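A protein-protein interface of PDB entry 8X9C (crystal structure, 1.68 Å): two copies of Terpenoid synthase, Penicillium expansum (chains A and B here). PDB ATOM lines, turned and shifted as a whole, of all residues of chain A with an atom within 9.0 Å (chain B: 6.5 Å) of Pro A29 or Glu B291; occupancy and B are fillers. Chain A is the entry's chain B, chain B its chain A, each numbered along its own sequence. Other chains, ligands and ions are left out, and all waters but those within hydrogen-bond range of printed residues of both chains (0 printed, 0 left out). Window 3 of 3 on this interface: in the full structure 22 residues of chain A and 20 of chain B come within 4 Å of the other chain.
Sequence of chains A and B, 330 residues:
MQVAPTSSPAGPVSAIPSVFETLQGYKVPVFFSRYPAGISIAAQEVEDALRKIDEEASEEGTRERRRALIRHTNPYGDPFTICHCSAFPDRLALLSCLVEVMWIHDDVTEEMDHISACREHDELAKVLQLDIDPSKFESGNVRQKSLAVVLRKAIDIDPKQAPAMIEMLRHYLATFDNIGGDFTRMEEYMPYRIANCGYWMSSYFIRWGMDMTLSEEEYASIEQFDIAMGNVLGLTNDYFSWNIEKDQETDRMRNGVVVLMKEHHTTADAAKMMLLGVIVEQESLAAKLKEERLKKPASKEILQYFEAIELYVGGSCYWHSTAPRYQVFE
The side-chain amide oxygen of Gln A24 sits at hydrogen-bond distance from the side-chain hydroxyl of Tyr A26, 2.9 Å away.
OE1 of Glu B283 sits at hydrogen-bond distance from N of Arg B34 (3.0 Å).
Of the 17 printed residues of chain A, 6 touch a printed residue of chain B.
Hydrophobic or aromatic side chains of chain A that line the printed part of chain B: Pro A29, Val A30 and Phe A32.
Of the 17 printed residues of chain B, 6 touch a printed residue of chain A.
Hydrophobic or aromatic side chains of chain B that line the printed part of chain A: Val B280 and Ala B287.
Among the printed residues, 11 pairs touch across the chains.
Among the printed residues, no Asp or Glu carboxylate lies within 4 Å of a Lys or Arg side-chain nitrogen of the other chain.
No position is printed for both chains.
Among the printed residues, merely in contact across the chains: Pro A29 with Lys B288, Val A30 with Ser B284, Pro A29 with Ala B287, Phe A32 with Val B280, Val A30 with Lys B288, Tyr A26 with Arg B34 and Pro A29 with Glu B291.
The backbone carbonyl oxygen of Pro A29 lies close to the side-chain hydroxyl of Ser B284, at 2.3 Å.
The backbone carbonyl oxygen (O) of Val A28 lies within hydrogen-bond range of the guanidinium group (NH2) of Arg B34 (3.0 Å).
The backbone carbonyl oxygen (O) of Phe A31 is in hydrogen-bond range of the guanidinium group (NH1) of Arg B34 (3.0 Å).
The guanidinium group (NH1) of Arg B34 sits at hydrogen-bond distance from the backbone carbonyl oxygen (O) of Pro A29 (2.9 Å).
Of the printed residues of chain A, Glu B291 touches Pro A29 (3.8 Å).
Printed residues of chain B within 4 Å of Phe A31: Arg B34 (3.0 Å).
Printed residues of chain B within 4 Å of Tyr A26: Arg B34.
Of the printed residues of chain B, Phe A32 touches Val B280 (3.7 Å).
Thr A322 touches none of the printed residues of chain B.
Leu B285 touches none of the printed residues of chain A.
The nearest residue of chain A that does not touch Glu B291 is Lys A27 (4.3 Å).
The nearest printed residue of chain B that does not touch Phe A32 is Arg B34 (4.5 Å).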
ATOM      1  N   GLN A  24      -9.197 -36.730 -16.142  1.00  0.00           N
ATOM      2  CA  GLN A  24      -9.830 -36.311 -14.866  1.00  0.00           C
ATOM      3  C   GLN A  24      -9.595 -34.811 -14.652  1.00  0.00           C
ATOM      4  O   GLN A  24      -8.645 -34.460 -13.955  1.00  0.00           O
ATOM      5  CB  GLN A  24      -9.255 -37.160 -13.732  1.00  0.00           C
ATOM      6  CG  GLN A  24      -9.041 -38.621 -14.092  1.00  0.00           C
ATOM      7  CD  GLN A  24      -8.250 -39.352 -13.034  1.00  0.00           C
ATOM      8  OE1 GLN A  24      -8.794 -39.820 -12.037  1.00  0.00           O
ATOM      9  NE2 GLN A  24      -6.947 -39.450 -13.243  1.00  0.00           N
ATOM     10  N   GLY A  25     -10.438 -33.966 -15.245  1.00  0.00           N
ATOM     11  CA  GLY A  25     -10.248 -32.508 -15.150  1.00  0.00           C
ATOM     12  C   GLY A  25     -10.440 -31.994 -13.739  1.00  0.00           C
ATOM     13  O   GLY A  25      -9.931 -30.918 -13.439  1.00  0.00           O
ATOM     14  N   TYR A  26     -11.154 -32.748 -12.912  1.00  0.00           N
ATOM     15  CA  TYR A  26     -11.350 -32.352 -11.495  1.00  0.00           C
ATOM     16  C   TYR A  26      -9.995 -32.095 -10.834  1.00  0.00           C
ATOM     17  O   TYR A  26      -9.944 -31.337  -9.859  1.00  0.00           O
ATOM     18  CB  TYR A  26     -12.155 -33.408 -10.729  1.00  0.00           C
ATOM     19  CG  TYR A  26     -11.461 -34.717 -10.455  1.00  0.00           C
ATOM     20  CD1 TYR A  26     -10.713 -34.904  -9.305  1.00  0.00           C
ATOM     21  CD2 TYR A  26     -11.582 -35.783 -11.327  1.00  0.00           C
ATOM     22  CE1 TYR A  26     -10.084 -36.110  -9.039  1.00  0.00           C
ATOM     23  CE2 TYR A  26     -10.965 -36.996 -11.074  1.00  0.00           C
ATOM     24  CZ  TYR A  26     -10.209 -37.159  -9.929  1.00  0.00           C
ATOM     25  OH  TYR A  26      -9.597 -38.352  -9.682  1.00  0.00           O
ATOM     26  N   LYS A  27      -8.940 -32.706 -11.355  1.00  0.00           N
ATOM     27  CA  LYS A  27      -7.593 -32.558 -10.758  1.00  0.00           C
ATOM     28  C   LYS A  27      -6.946 -31.243 -11.208  1.00  0.00           C
ATOM     29  O   LYS A  27      -5.856 -30.945 -10.710  1.00  0.00           O
ATOM     30  CB  LYS A  27      -6.763 -33.779 -11.151  1.00  0.00           C
ATOM     31  CG  LYS A  27      -7.300 -35.109 -10.646  1.00  0.00           C
ATOM     32  CD  LYS A  27      -6.688 -36.299 -11.347  1.00  0.00           C
ATOM     33  CE  LYS A  27      -6.628 -37.534 -10.474  1.00  0.00           C
ATOM     34  NZ  LYS A  27      -5.362 -38.278 -10.667  1.00  0.00           N
ATOM     35  N   VAL A  28      -7.584 -30.495 -12.114  1.00  0.00           N
ATOM     36  CA  VAL A  28      -7.049 -29.233 -12.615  1.00  0.00           C
ATOM     37  C   VAL A  28      -7.896 -28.109 -12.031  1.00  0.00           C
ATOM     38  O   VAL A  28      -9.047 -27.923 -12.452  1.00  0.00           O
ATOM     39  CB  VAL A  28      -7.042 -29.185 -14.149  1.00  0.00           C
ATOM     40  CG1 VAL A  28      -6.297 -27.958 -14.634  1.00  0.00           C
ATOM     41  CG2 VAL A  28      -6.391 -30.458 -14.712  1.00  0.00           C
ATOM     42  N   PRO A  29      -7.385 -27.344 -11.063  1.00  0.00           N
ATOM     43  CA  PRO A  29      -8.228 -26.337 -10.406  1.00  0.00           C
ATOM     44  C   PRO A  29      -8.775 -25.262 -11.339  1.00  0.00           C
ATOM     45  O   PRO A  29      -9.890 -24.780 -11.113  1.00  0.00           O
ATOM     46  CB  PRO A  29      -7.293 -25.751  -9.340  1.00  0.00           C
ATOM     47  CG  PRO A  29      -6.388 -26.891  -8.988  1.00  0.00           C
ATOM     48  CD  PRO A  29      -6.116 -27.560 -10.339  1.00  0.00           C
ATOM     49  N   VAL A  30      -8.076 -24.933 -12.420  1.00  0.00           N
ATOM     50  CA  VAL A  30      -8.531 -23.838 -13.329  1.00  0.00           C
ATOM     51  C   VAL A  30      -9.596 -24.374 -14.292  1.00  0.00           C
ATOM     52  O   VAL A  30     -10.310 -23.573 -14.876  1.00  0.00           O
ATOM     53  CB  VAL A  30      -7.354 -23.217 -14.102  1.00  0.00           C
ATOM     54  CG1 VAL A  30      -6.435 -22.437 -13.179  1.00  0.00           C
ATOM     55  CG2 VAL A  30      -6.578 -24.269 -14.865  1.00  0.00           C
ATOM     56  N   PHE A  31      -9.670 -25.690 -14.440  1.00  0.00           N
ATOM     57  CA  PHE A  31     -10.665 -26.299 -15.317  1.00  0.00           C
ATOM     58  C   PHE A  31     -12.049 -26.183 -14.684  1.00  0.00           C
ATOM     59  O   PHE A  31     -12.297 -26.764 -13.626  1.00  0.00           O
ATOM     60  CB  PHE A  31     -10.285 -27.762 -15.562  1.00  0.00           C
ATOM     61  CG  PHE A  31     -11.309 -28.541 -16.332  1.00  0.00           C
ATOM     62  CD1 PHE A  31     -11.436 -28.380 -17.703  1.00  0.00           C
ATOM     63  CD2 PHE A  31     -12.163 -29.422 -15.678  1.00  0.00           C
ATOM     64  CE1 PHE A  31     -12.375 -29.103 -18.412  1.00  0.00           C
ATOM     65  CE2 PHE A  31     -13.113 -30.142 -16.384  1.00  0.00           C
ATOM     66  CZ  PHE A  31     -13.212 -29.981 -17.768  1.00  0.00           C
ATOM     67  N   PHE A  32     -12.957 -25.431 -15.322  1.00  0.00           N
ATOM     68  CA  PHE A  32     -14.272 -25.175 -14.746  1.00  0.00           C
ATOM     69  C   PHE A  32     -15.435 -25.813 -15.502  1.00  0.00           C
ATOM     70  O   PHE A  32     -16.579 -25.733 -15.031  1.00  0.00           O
ATOM     71  CB  PHE A  32     -14.512 -23.662 -14.660  1.00  0.00           C
ATOM     72  CG  PHE A  32     -14.552 -22.985 -16.003  1.00  0.00           C
ATOM     73  CD1 PHE A  32     -15.718 -22.960 -16.749  1.00  0.00           C
ATOM     74  CD2 PHE A  32     -13.430 -22.346 -16.498  1.00  0.00           C
ATOM     75  CE1 PHE A  32     -15.753 -22.329 -17.983  1.00  0.00           C
ATOM     76  CE2 PHE A  32     -13.454 -21.707 -17.733  1.00  0.00           C
ATOM     77  CZ  PHE A  32     -14.618 -21.698 -18.477  1.00  0.00           C
ATOM     78  N   SER A  33     -15.193 -26.413 -16.660  1.00  0.00           N
ATOM     79  CA  SER A  33     -16.293 -26.882 -17.485  1.00  0.00           C
ATOM     80  C   SER A  33     -17.040 -28.026 -16.822  1.00  0.00           C
ATOM     81  O   SER A  33     -16.454 -28.858 -16.125  1.00  0.00           O
ATOM     82  CB  SER A  33     -15.774 -27.360 -18.846  1.00  0.00           C
ATOM     83  OG  SER A  33     -16.859 -27.736 -19.674  1.00  0.00           O
ATOM     84  N   TYR A  76       0.185 -31.487 -21.170  1.00  0.00           N
ATOM     85  CA  TYR A  76      -1.044 -32.203 -20.752  1.00  0.00           C
ATOM     86  C   TYR A  76      -1.764 -32.734 -21.983  1.00  0.00           C
ATOM     87  O   TYR A  76      -2.705 -33.522 -21.849  1.00  0.00           O
ATOM     88  CB  TYR A  76      -1.953 -31.278 -19.948  1.00  0.00           C
ATOM     89  CG  TYR A  76      -1.448 -31.011 -18.556  1.00  0.00           C
ATOM     90  CD1 TYR A  76      -0.468 -30.062 -18.328  1.00  0.00           C
ATOM     91  CD2 TYR A  76      -1.930 -31.725 -17.474  1.00  0.00           C
ATOM     92  CE1 TYR A  76       0.011 -29.818 -17.053  1.00  0.00           C
ATOM     93  CE2 TYR A  76      -1.464 -31.491 -16.192  1.00  0.00           C
ATOM     94  CZ  TYR A  76      -0.489 -30.534 -15.983  1.00  0.00           C
ATOM     95  OH  TYR A  76      -0.021 -30.294 -14.725  1.00  0.00           O
ATOM     96  N   TYR A 239     -11.671 -16.189 -22.624  1.00  0.00           N
ATOM     97  CA  TYR A 239     -11.429 -16.091 -21.189  1.00  0.00           C
ATOM     98  C   TYR A 239      -9.979 -16.425 -20.864  1.00  0.00           C
ATOM     99  O   TYR A 239      -9.306 -15.685 -20.139  1.00  0.00           O
ATOM    100  CB  TYR A 239     -12.389 -17.004 -20.425  1.00  0.00           C
ATOM    101  CG  TYR A 239     -12.167 -16.982 -18.929  1.00  0.00           C
ATOM    102  CD1 TYR A 239     -12.731 -15.978 -18.153  1.00  0.00           C
ATOM    103  CD2 TYR A 239     -11.411 -17.964 -18.298  1.00  0.00           C
ATOM    104  CE1 TYR A 239     -12.544 -15.945 -16.782  1.00  0.00           C
ATOM    105  CE2 TYR A 239     -11.213 -17.936 -16.928  1.00  0.00           C
ATOM    106  CZ  TYR A 239     -11.783 -16.923 -16.187  1.00  0.00           C
ATOM    107  OH  TYR A 239     -11.590 -16.896 -14.822  1.00  0.00           O
ATOM    108  N   PHE A 240      -9.460 -17.515 -21.439  1.00  0.00           N
ATOM    109  CA  PHE A 240      -8.109 -17.927 -21.100  1.00  0.00           C
ATOM    110  C   PHE A 240      -7.042 -17.135 -21.831  1.00  0.00           C
ATOM    111  O   PHE A 240      -5.891 -17.126 -21.386  1.00  0.00           O
ATOM    112  CB  PHE A 240      -7.925 -19.419 -21.362  1.00  0.00           C
ATOM    113  CG  PHE A 240      -8.565 -20.275 -20.325  1.00  0.00           C
ATOM    114  CD1 PHE A 240      -8.003 -20.382 -19.060  1.00  0.00           C
ATOM    115  CD2 PHE A 240      -9.725 -20.971 -20.600  1.00  0.00           C
ATOM    116  CE1 PHE A 240      -8.598 -21.158 -18.095  1.00  0.00           C
ATOM    117  CE2 PHE A 240     -10.318 -21.764 -19.638  1.00  0.00           C
ATOM    118  CZ  PHE A 240      -9.755 -21.857 -18.385  1.00  0.00           C
ATOM    119  N   CYS A 317     -11.822 -26.744 -22.971  1.00  0.00           N
ATOM    120  CA  CYS A 317     -11.623 -26.070 -21.691  1.00  0.00           C
ATOM    121  C   CYS A 317     -10.415 -26.638 -20.961  1.00  0.00           C
ATOM    122  O   CYS A 317      -9.596 -25.888 -20.415  1.00  0.00           O
ATOM    123  CB  CYS A 317     -12.875 -26.194 -20.827  1.00  0.00           C
ATOM    124  SG  CYS A 317     -12.711 -25.199 -19.325  1.00  0.00           S
ATOM    125  N   TYR A 318     -10.269 -27.962 -20.991  1.00  0.00           N
ATOM    126  CA  TYR A 318      -9.145 -28.625 -20.348  1.00  0.00           C
ATOM    127  C   TYR A 318      -7.822 -28.206 -20.972  1.00  0.00           C
ATOM    128  O   TYR A 318      -6.854 -27.911 -20.259  1.00  0.00           O
ATOM    129  CB  TYR A 318      -9.353 -30.131 -20.438  1.00  0.00           C
ATOM    130  CG  TYR A 318      -8.287 -30.975 -19.781  1.00  0.00           C
ATOM    131  CD1 TYR A 318      -7.161 -31.381 -20.492  1.00  0.00           C
ATOM    132  CD2 TYR A 318      -8.399 -31.348 -18.447  1.00  0.00           C
ATOM    133  CE1 TYR A 318      -6.184 -32.156 -19.892  1.00  0.00           C
ATOM    134  CE2 TYR A 318      -7.428 -32.121 -17.840  1.00  0.00           C
ATOM    135  CZ  TYR A 318      -6.327 -32.520 -18.567  1.00  0.00           C
ATOM    136  OH  TYR A 318      -5.356 -33.287 -17.961  1.00  0.00           O
ATOM    137  N   SER A 321      -7.023 -24.781 -20.042  1.00  0.00           N
ATOM    138  CA  SER A 321      -6.788 -24.705 -18.603  1.00  0.00           C
ATOM    139  C   SER A 321      -5.372 -25.118 -18.236  1.00  0.00           C
ATOM    140  O   SER A 321      -4.817 -24.615 -17.251  1.00  0.00           O
ATOM    141  CB  SER A 321      -7.784 -25.596 -17.867  1.00  0.00           C
ATOM    142  OG  SER A 321      -9.088 -25.058 -17.939  1.00  0.00           O
ATOM    143  N   THR A 322      -4.783 -26.037 -18.996  1.00  0.00           N
ATOM    144  CA  THR A 322      -3.486 -26.619 -18.680  1.00  0.00           C
ATOM    145  C   THR A 322      -2.354 -26.084 -19.546  1.00  0.00           C
ATOM    146  O   THR A 322      -1.205 -26.492 -19.349  1.00  0.00           O
ATOM    147  CB  THR A 322      -3.548 -28.141 -18.828  1.00  0.00           C
ATOM    148  OG1 THR A 322      -4.032 -28.463 -20.136  1.00  0.00           O
ATOM    149  CG2 THR A 322      -4.478 -28.756 -17.797  1.00  0.00           C
ATOM    150  N   ARG B  34     -18.545 -27.530  -9.444  1.00  0.00           N
ATOM    151  CA  ARG B  34     -17.550 -28.582  -9.637  1.00  0.00           C
ATOM    152  C   ARG B  34     -17.527 -29.590  -8.495  1.00  0.00           C
ATOM    153  O   ARG B  34     -16.852 -30.627  -8.605  1.00  0.00           O
ATOM    154  CB  ARG B  34     -16.172 -27.936  -9.801  1.00  0.00           C
ATOM    155  CG  ARG B  34     -15.581 -27.466  -8.476  1.00  0.00           C
ATOM    156  CD  ARG B  34     -14.282 -26.708  -8.681  1.00  0.00           C
ATOM    157  NE  ARG B  34     -13.264 -27.548  -9.293  1.00  0.00           N
ATOM    158  CZ  ARG B  34     -12.419 -27.135 -10.225  1.00  0.00           C
ATOM    159  NH1 ARG B  34     -12.489 -25.911 -10.728  1.00  0.00           N
ATOM    160  NH2 ARG B  34     -11.486 -27.972 -10.667  1.00  0.00           N
ATOM    161  N   VAL B 280     -17.548 -19.090  -9.477  1.00  0.00           N
ATOM    162  CA  VAL B 280     -16.775 -20.177 -10.148  1.00  0.00           C
ATOM    163  C   VAL B 280     -15.283 -20.006  -9.833  1.00  0.00           C
ATOM    164  O   VAL B 280     -14.610 -21.002  -9.581  1.00  0.00           O
ATOM    165  CB  VAL B 280     -17.059 -20.201 -11.661  1.00  0.00           C
ATOM    166  CG1 VAL B 280     -16.138 -21.150 -12.406  1.00  0.00           C
ATOM    167  CG2 VAL B 280     -18.514 -20.534 -11.943  1.00  0.00           C
ATOM    168  N   GLU B 283     -14.671 -21.251  -6.460  1.00  0.00           N
ATOM    169  CA  GLU B 283     -14.613 -22.707  -6.455  1.00  0.00           C
ATOM    170  C   GLU B 283     -13.250 -23.182  -6.950  1.00  0.00           C
ATOM    171  O   GLU B 283     -12.681 -24.142  -6.416  1.00  0.00           O
ATOM    172  CB  GLU B 283     -15.738 -23.296  -7.320  1.00  0.00           C
ATOM    173  CG  GLU B 283     -17.120 -23.318  -6.634  1.00  0.00           C
ATOM    174  CD  GLU B 283     -18.114 -24.284  -7.270  1.00  0.00           C
ATOM    175  OE1 GLU B 283     -17.814 -24.859  -8.345  1.00  0.00           O
ATOM    176  OE2 GLU B 283     -19.182 -24.535  -6.657  1.00  0.00           O
ATOM    177  N   SER B 284     -12.704 -22.502  -7.968  1.00  0.00           N
ATOM    178  CA  SER B 284     -11.355 -22.797  -8.443  1.00  0.00           C
ATOM    179  C   SER B 284     -10.302 -22.473  -7.390  1.00  0.00           C
ATOM    180  O   SER B 284      -9.365 -23.254  -7.178  1.00  0.00           O
ATOM    181  CB  SER B 284     -11.084 -22.010  -9.728  1.00  0.00           C
ATOM    182  OG  SER B 284      -9.987 -22.564 -10.414  1.00  0.00           O
ATOM    183  N   LEU B 285     -10.432 -21.315  -6.734  1.00  0.00           N
ATOM    184  CA  LEU B 285      -9.492 -20.938  -5.684  1.00  0.00           C
ATOM    185  C   LEU B 285      -9.443 -21.986  -4.585  1.00  0.00           C
ATOM    186  O   LEU B 285      -8.359 -22.360  -4.123  1.00  0.00           O
ATOM    187  CB  LEU B 285      -9.879 -19.581  -5.090  1.00  0.00           C
ATOM    188  CG  LEU B 285      -8.910 -19.034  -4.032  1.00  0.00           C
ATOM    189  CD1 LEU B 285      -7.469 -18.935  -4.523  1.00  0.00           C
ATOM    190  CD2 LEU B 285      -9.425 -17.705  -3.472  1.00  0.00           C
ATOM    191  N   ALA B 286     -10.614 -22.467  -4.151  1.00  0.00           N
ATOM    192  CA  ALA B 286     -10.653 -23.514  -3.141  1.00  0.00           C
ATOM    193  C   ALA B 286      -9.902 -24.745  -3.616  1.00  0.00           C
ATOM    194  O   ALA B 286      -9.136 -25.343  -2.855  1.00  0.00           O
ATOM    195  CB  ALA B 286     -12.101 -23.867  -2.793  1.00  0.00           C
ATOM    196  N   ALA B 287     -10.089 -25.123  -4.882  1.00  0.00           N
ATOM    197  CA  ALA B 287      -9.382 -26.282  -5.411  1.00  0.00           C
ATOM    198  C   ALA B 287      -7.873 -26.048  -5.427  1.00  0.00           C
ATOM    199  O   ALA B 287      -7.098 -26.972  -5.137  1.00  0.00           O
ATOM    200  CB  ALA B 287      -9.904 -26.622  -6.808  1.00  0.00           C
ATOM    201  N   LYS B 288      -7.446 -24.828  -5.716  1.00  0.00           N
ATOM    202  CA  LYS B 288      -5.994 -24.532  -5.709  1.00  0.00           C
ATOM    203  C   LYS B 288      -5.477 -24.635  -4.274  1.00  0.00           C
ATOM    204  O   LYS B 288      -4.458 -25.287  -4.064  1.00  0.00           O
ATOM    205  CB  LYS B 288      -5.709 -23.152  -6.300  1.00  0.00           C
ATOM    206  CG  LYS B 288      -6.206 -22.924  -7.718  1.00  0.00           C
ATOM    207  CD  LYS B 288      -6.358 -21.460  -8.053  1.00  0.00           C
ATOM    208  CE  LYS B 288      -6.723 -21.215  -9.500  1.00  0.00           C
ATOM    209  NZ  LYS B 288      -5.763 -20.298 -10.152  1.00  0.00           N
ATOM    210  N   LEU B 289      -6.191 -24.029  -3.331  1.00  0.00           N
ATOM    211  CA  LEU B 289      -5.739 -24.047  -1.946  1.00  0.00           C
ATOM    212  C   LEU B 289      -5.687 -25.465  -1.387  1.00  0.00           C
ATOM    213  O   LEU B 289      -4.795 -25.793  -0.596  1.00  0.00           O
ATOM    214  CB  LEU B 289      -6.654 -23.156  -1.115  1.00  0.00           C
ATOM    215  CG  LEU B 289      -6.553 -21.690  -1.514  1.00  0.00           C
ATOM    216  CD1 LEU B 289      -7.638 -20.856  -0.863  1.00  0.00           C
ATOM    217  CD2 LEU B 289      -5.183 -21.173  -1.112  1.00  0.00           C
ATOM    218  N   LYS B 290      -6.643 -26.317  -1.764  1.00  0.00           N
ATOM    219  CA  LYS B 290      -6.598 -27.707  -1.328  1.00  0.00           C
ATOM    220  C   LYS B 290      -5.393 -28.428  -1.918  1.00  0.00           C
ATOM    221  O   LYS B 290      -4.722 -29.206  -1.232  1.00  0.00           O
ATOM    222  CB  LYS B 290      -7.883 -28.420  -1.731  1.00  0.00           C
ATOM    223  CG  LYS B 290      -7.878 -29.906  -1.481  1.00  0.00           C
ATOM    224  CD  LYS B 290      -9.142 -30.522  -2.031  1.00  0.00           C
ATOM    225  CE  LYS B 290      -9.172 -32.012  -1.908  1.00  0.00           C
ATOM    226  NZ  LYS B 290     -10.381 -32.552  -2.582  1.00  0.00           N
ATOM    227  N   GLU B 291      -5.117 -28.188  -3.199  1.00  0.00           N
ATOM    228  CA  GLU B 291      -3.954 -28.806  -3.827  1.00  0.00           C
ATOM    229  C   GLU B 291      -2.661 -28.325  -3.173  1.00  0.00           C
ATOM    230  O   GLU B 291      -1.720 -29.108  -2.997  1.00  0.00           O
ATOM    231  CB  GLU B 291      -3.979 -28.519  -5.330  1.00  0.00           C
ATOM    232  CG  GLU B 291      -2.653 -28.159  -5.979  1.00  0.00           C
ATOM    233  CD  GLU B 291      -2.817 -27.845  -7.466  1.00  0.00           C
ATOM    234  OE1 GLU B 291      -3.119 -28.775  -8.245  1.00  0.00           O
ATOM    235  OE2 GLU B 291      -2.673 -26.658  -7.847  1.00  0.00           O
ATOM    236  N   GLU B 292      -2.643 -27.066  -2.747  1.00  0.00           N
ATOM    237  CA  GLU B 292      -1.451 -26.532  -2.044  1.00  0.00           C
ATOM    238  C   GLU B 292      -1.290 -27.249  -0.698  1.00  0.00           C
ATOM    239  O   GLU B 292      -0.163 -27.637  -0.382  1.00  0.00           O
ATOM    240  CB  GLU B 292      -1.556 -25.021  -1.870  1.00  0.00           C
ATOM    241  CG  GLU B 292      -1.317 -24.252  -3.151  1.00  0.00           C
ATOM    242  CD  GLU B 292      -0.007 -24.585  -3.843  1.00  0.00           C
ATOM    243  OE1 GLU B 292       1.038 -24.555  -3.168  1.00  0.00           O
ATOM    244  OE2 GLU B 292      -0.037 -24.877  -5.053  1.00  0.00           O
ATOM    245  N   ARG B 293      -2.374 -27.420   0.060  1.00  0.00           N
ATOM    246  CA  ARG B 293      -2.268 -28.058   1.372  1.00  0.00           C
ATOM    247  C   ARG B 293      -1.843 -29.517   1.252  1.00  0.00           C
ATOM    248  O   ARG B 293      -1.059 -30.011   2.073  1.00  0.00           O
ATOM    249  CB  ARG B 293      -3.598 -27.955   2.118  1.00  0.00           C
ATOM    250  CG  ARG B 293      -3.634 -28.727   3.439  1.00  0.00           C
ATOM    251  CD  ARG B 293      -2.628 -28.153   4.427  1.00  0.00           C
ATOM    252  NE  ARG B 293      -2.610 -28.848   5.713  1.00  0.00           N
ATOM    253  CZ  ARG B 293      -2.162 -30.080   5.914  1.00  0.00           C
ATOM    254  NH1 ARG B 293      -1.663 -30.807   4.927  1.00  0.00           N
ATOM    255  NH2 ARG B 293      -2.189 -30.588   7.144  1.00  0.00           N
ATOM    256  N   LEU B 294      -2.338 -30.222   0.232  1.00  0.00           N
ATOM    257  CA  LEU B 294      -2.062 -31.646   0.065  1.00  0.00           C
ATOM    258  C   LEU B 294      -0.648 -31.929  -0.434  1.00  0.00           C
ATOM    259  O   LEU B 294      -0.297 -33.101  -0.588  1.00  0.00           O
ATOM    260  CB  LEU B 294      -3.096 -32.269  -0.880  1.00  0.00           C
ATOM    261  CG  LEU B 294      -4.519 -32.406  -0.312  1.00  0.00           C
ATOM    262  CD1 LEU B 294      -5.319 -33.464  -1.055  1.00  0.00           C
ATOM    263  CD2 LEU B 294      -4.458 -32.752   1.170  1.00  0.00           C
ATOM    264  N   LYS B 295       0.171 -30.895  -0.584  1.00  0.00           N
ATOM    265  CA  LYS B 295       1.599 -31.123  -0.914  1.00  0.00           C
ATOM    266  C   LYS B 295       2.316 -31.514   0.384  1.00  0.00           C
ATOM    267  O   LYS B 295       3.399 -32.102   0.283  1.00  0.00           O
ATOM    268  CB  LYS B 295       2.191 -29.861  -1.532  1.00  0.00           C
ATOM    269  CG  LYS B 295       1.585 -29.418  -2.854  1.00  0.00           C
ATOM    270  CD  LYS B 295       1.793 -27.943  -3.100  1.00  0.00           C
ATOM    271  CE  LYS B 295       2.326 -27.636  -4.482  1.00  0.00           C
ATOM    272  NZ  LYS B 295       2.796 -26.235  -4.583  1.00  0.00           N
ATOM    273  N   LYS B 296       1.743 -31.187   1.545  1.00  0.00           N
ATOM    274  CA  LYS B 296       2.271 -31.538   2.853  1.00  0.00           C
ATOM    275  C   LYS B 296       1.471 -32.686   3.447  1.00  0.00           C
ATOM    276  O   LYS B 296       0.334 -32.939   3.040  1.00  0.00           O
ATOM    277  CB  LYS B 296       2.221 -30.322   3.789  1.00  0.00           C
ATOM    278  CG  LYS B 296       3.331 -29.303   3.529  1.00  0.00           C
ATOM    279  CD  LYS B 296       3.816 -28.637   4.816  1.00  0.00           C
ATOM    280  CE  LYS B 296       3.360 -27.190   4.916  1.00  0.00           C
ATOM    281  NZ  LYS B 296       3.698 -26.594   6.245  1.00  0.00           N
ATOM    282  N   PHE B 306     -12.074 -32.010   4.004  1.00  0.00           N
ATOM    283  CA  PHE B 306     -12.079 -31.660   2.567  1.00  0.00           C
ATOM    284  C   PHE B 306     -13.244 -32.387   1.896  1.00  0.00           C
ATOM    285  O   PHE B 306     -14.030 -31.733   1.219  1.00  0.00           O
ATOM    286  CB  PHE B 306     -10.758 -32.032   1.897  1.00  0.00           C
ATOM    287  CG  PHE B 306      -9.625 -31.057   2.074  1.00  0.00           C
ATOM    288  CD1 PHE B 306      -9.849 -29.692   2.055  1.00  0.00           C
ATOM    289  CD2 PHE B 306      -8.327 -31.510   2.235  1.00  0.00           C
ATOM    290  CE1 PHE B 306      -8.800 -28.802   2.209  1.00  0.00           C
ATOM    291  CE2 PHE B 306      -7.280 -30.619   2.386  1.00  0.00           C
ATOM    292  CZ  PHE B 306      -7.518 -29.266   2.374  1.00  0.00           C
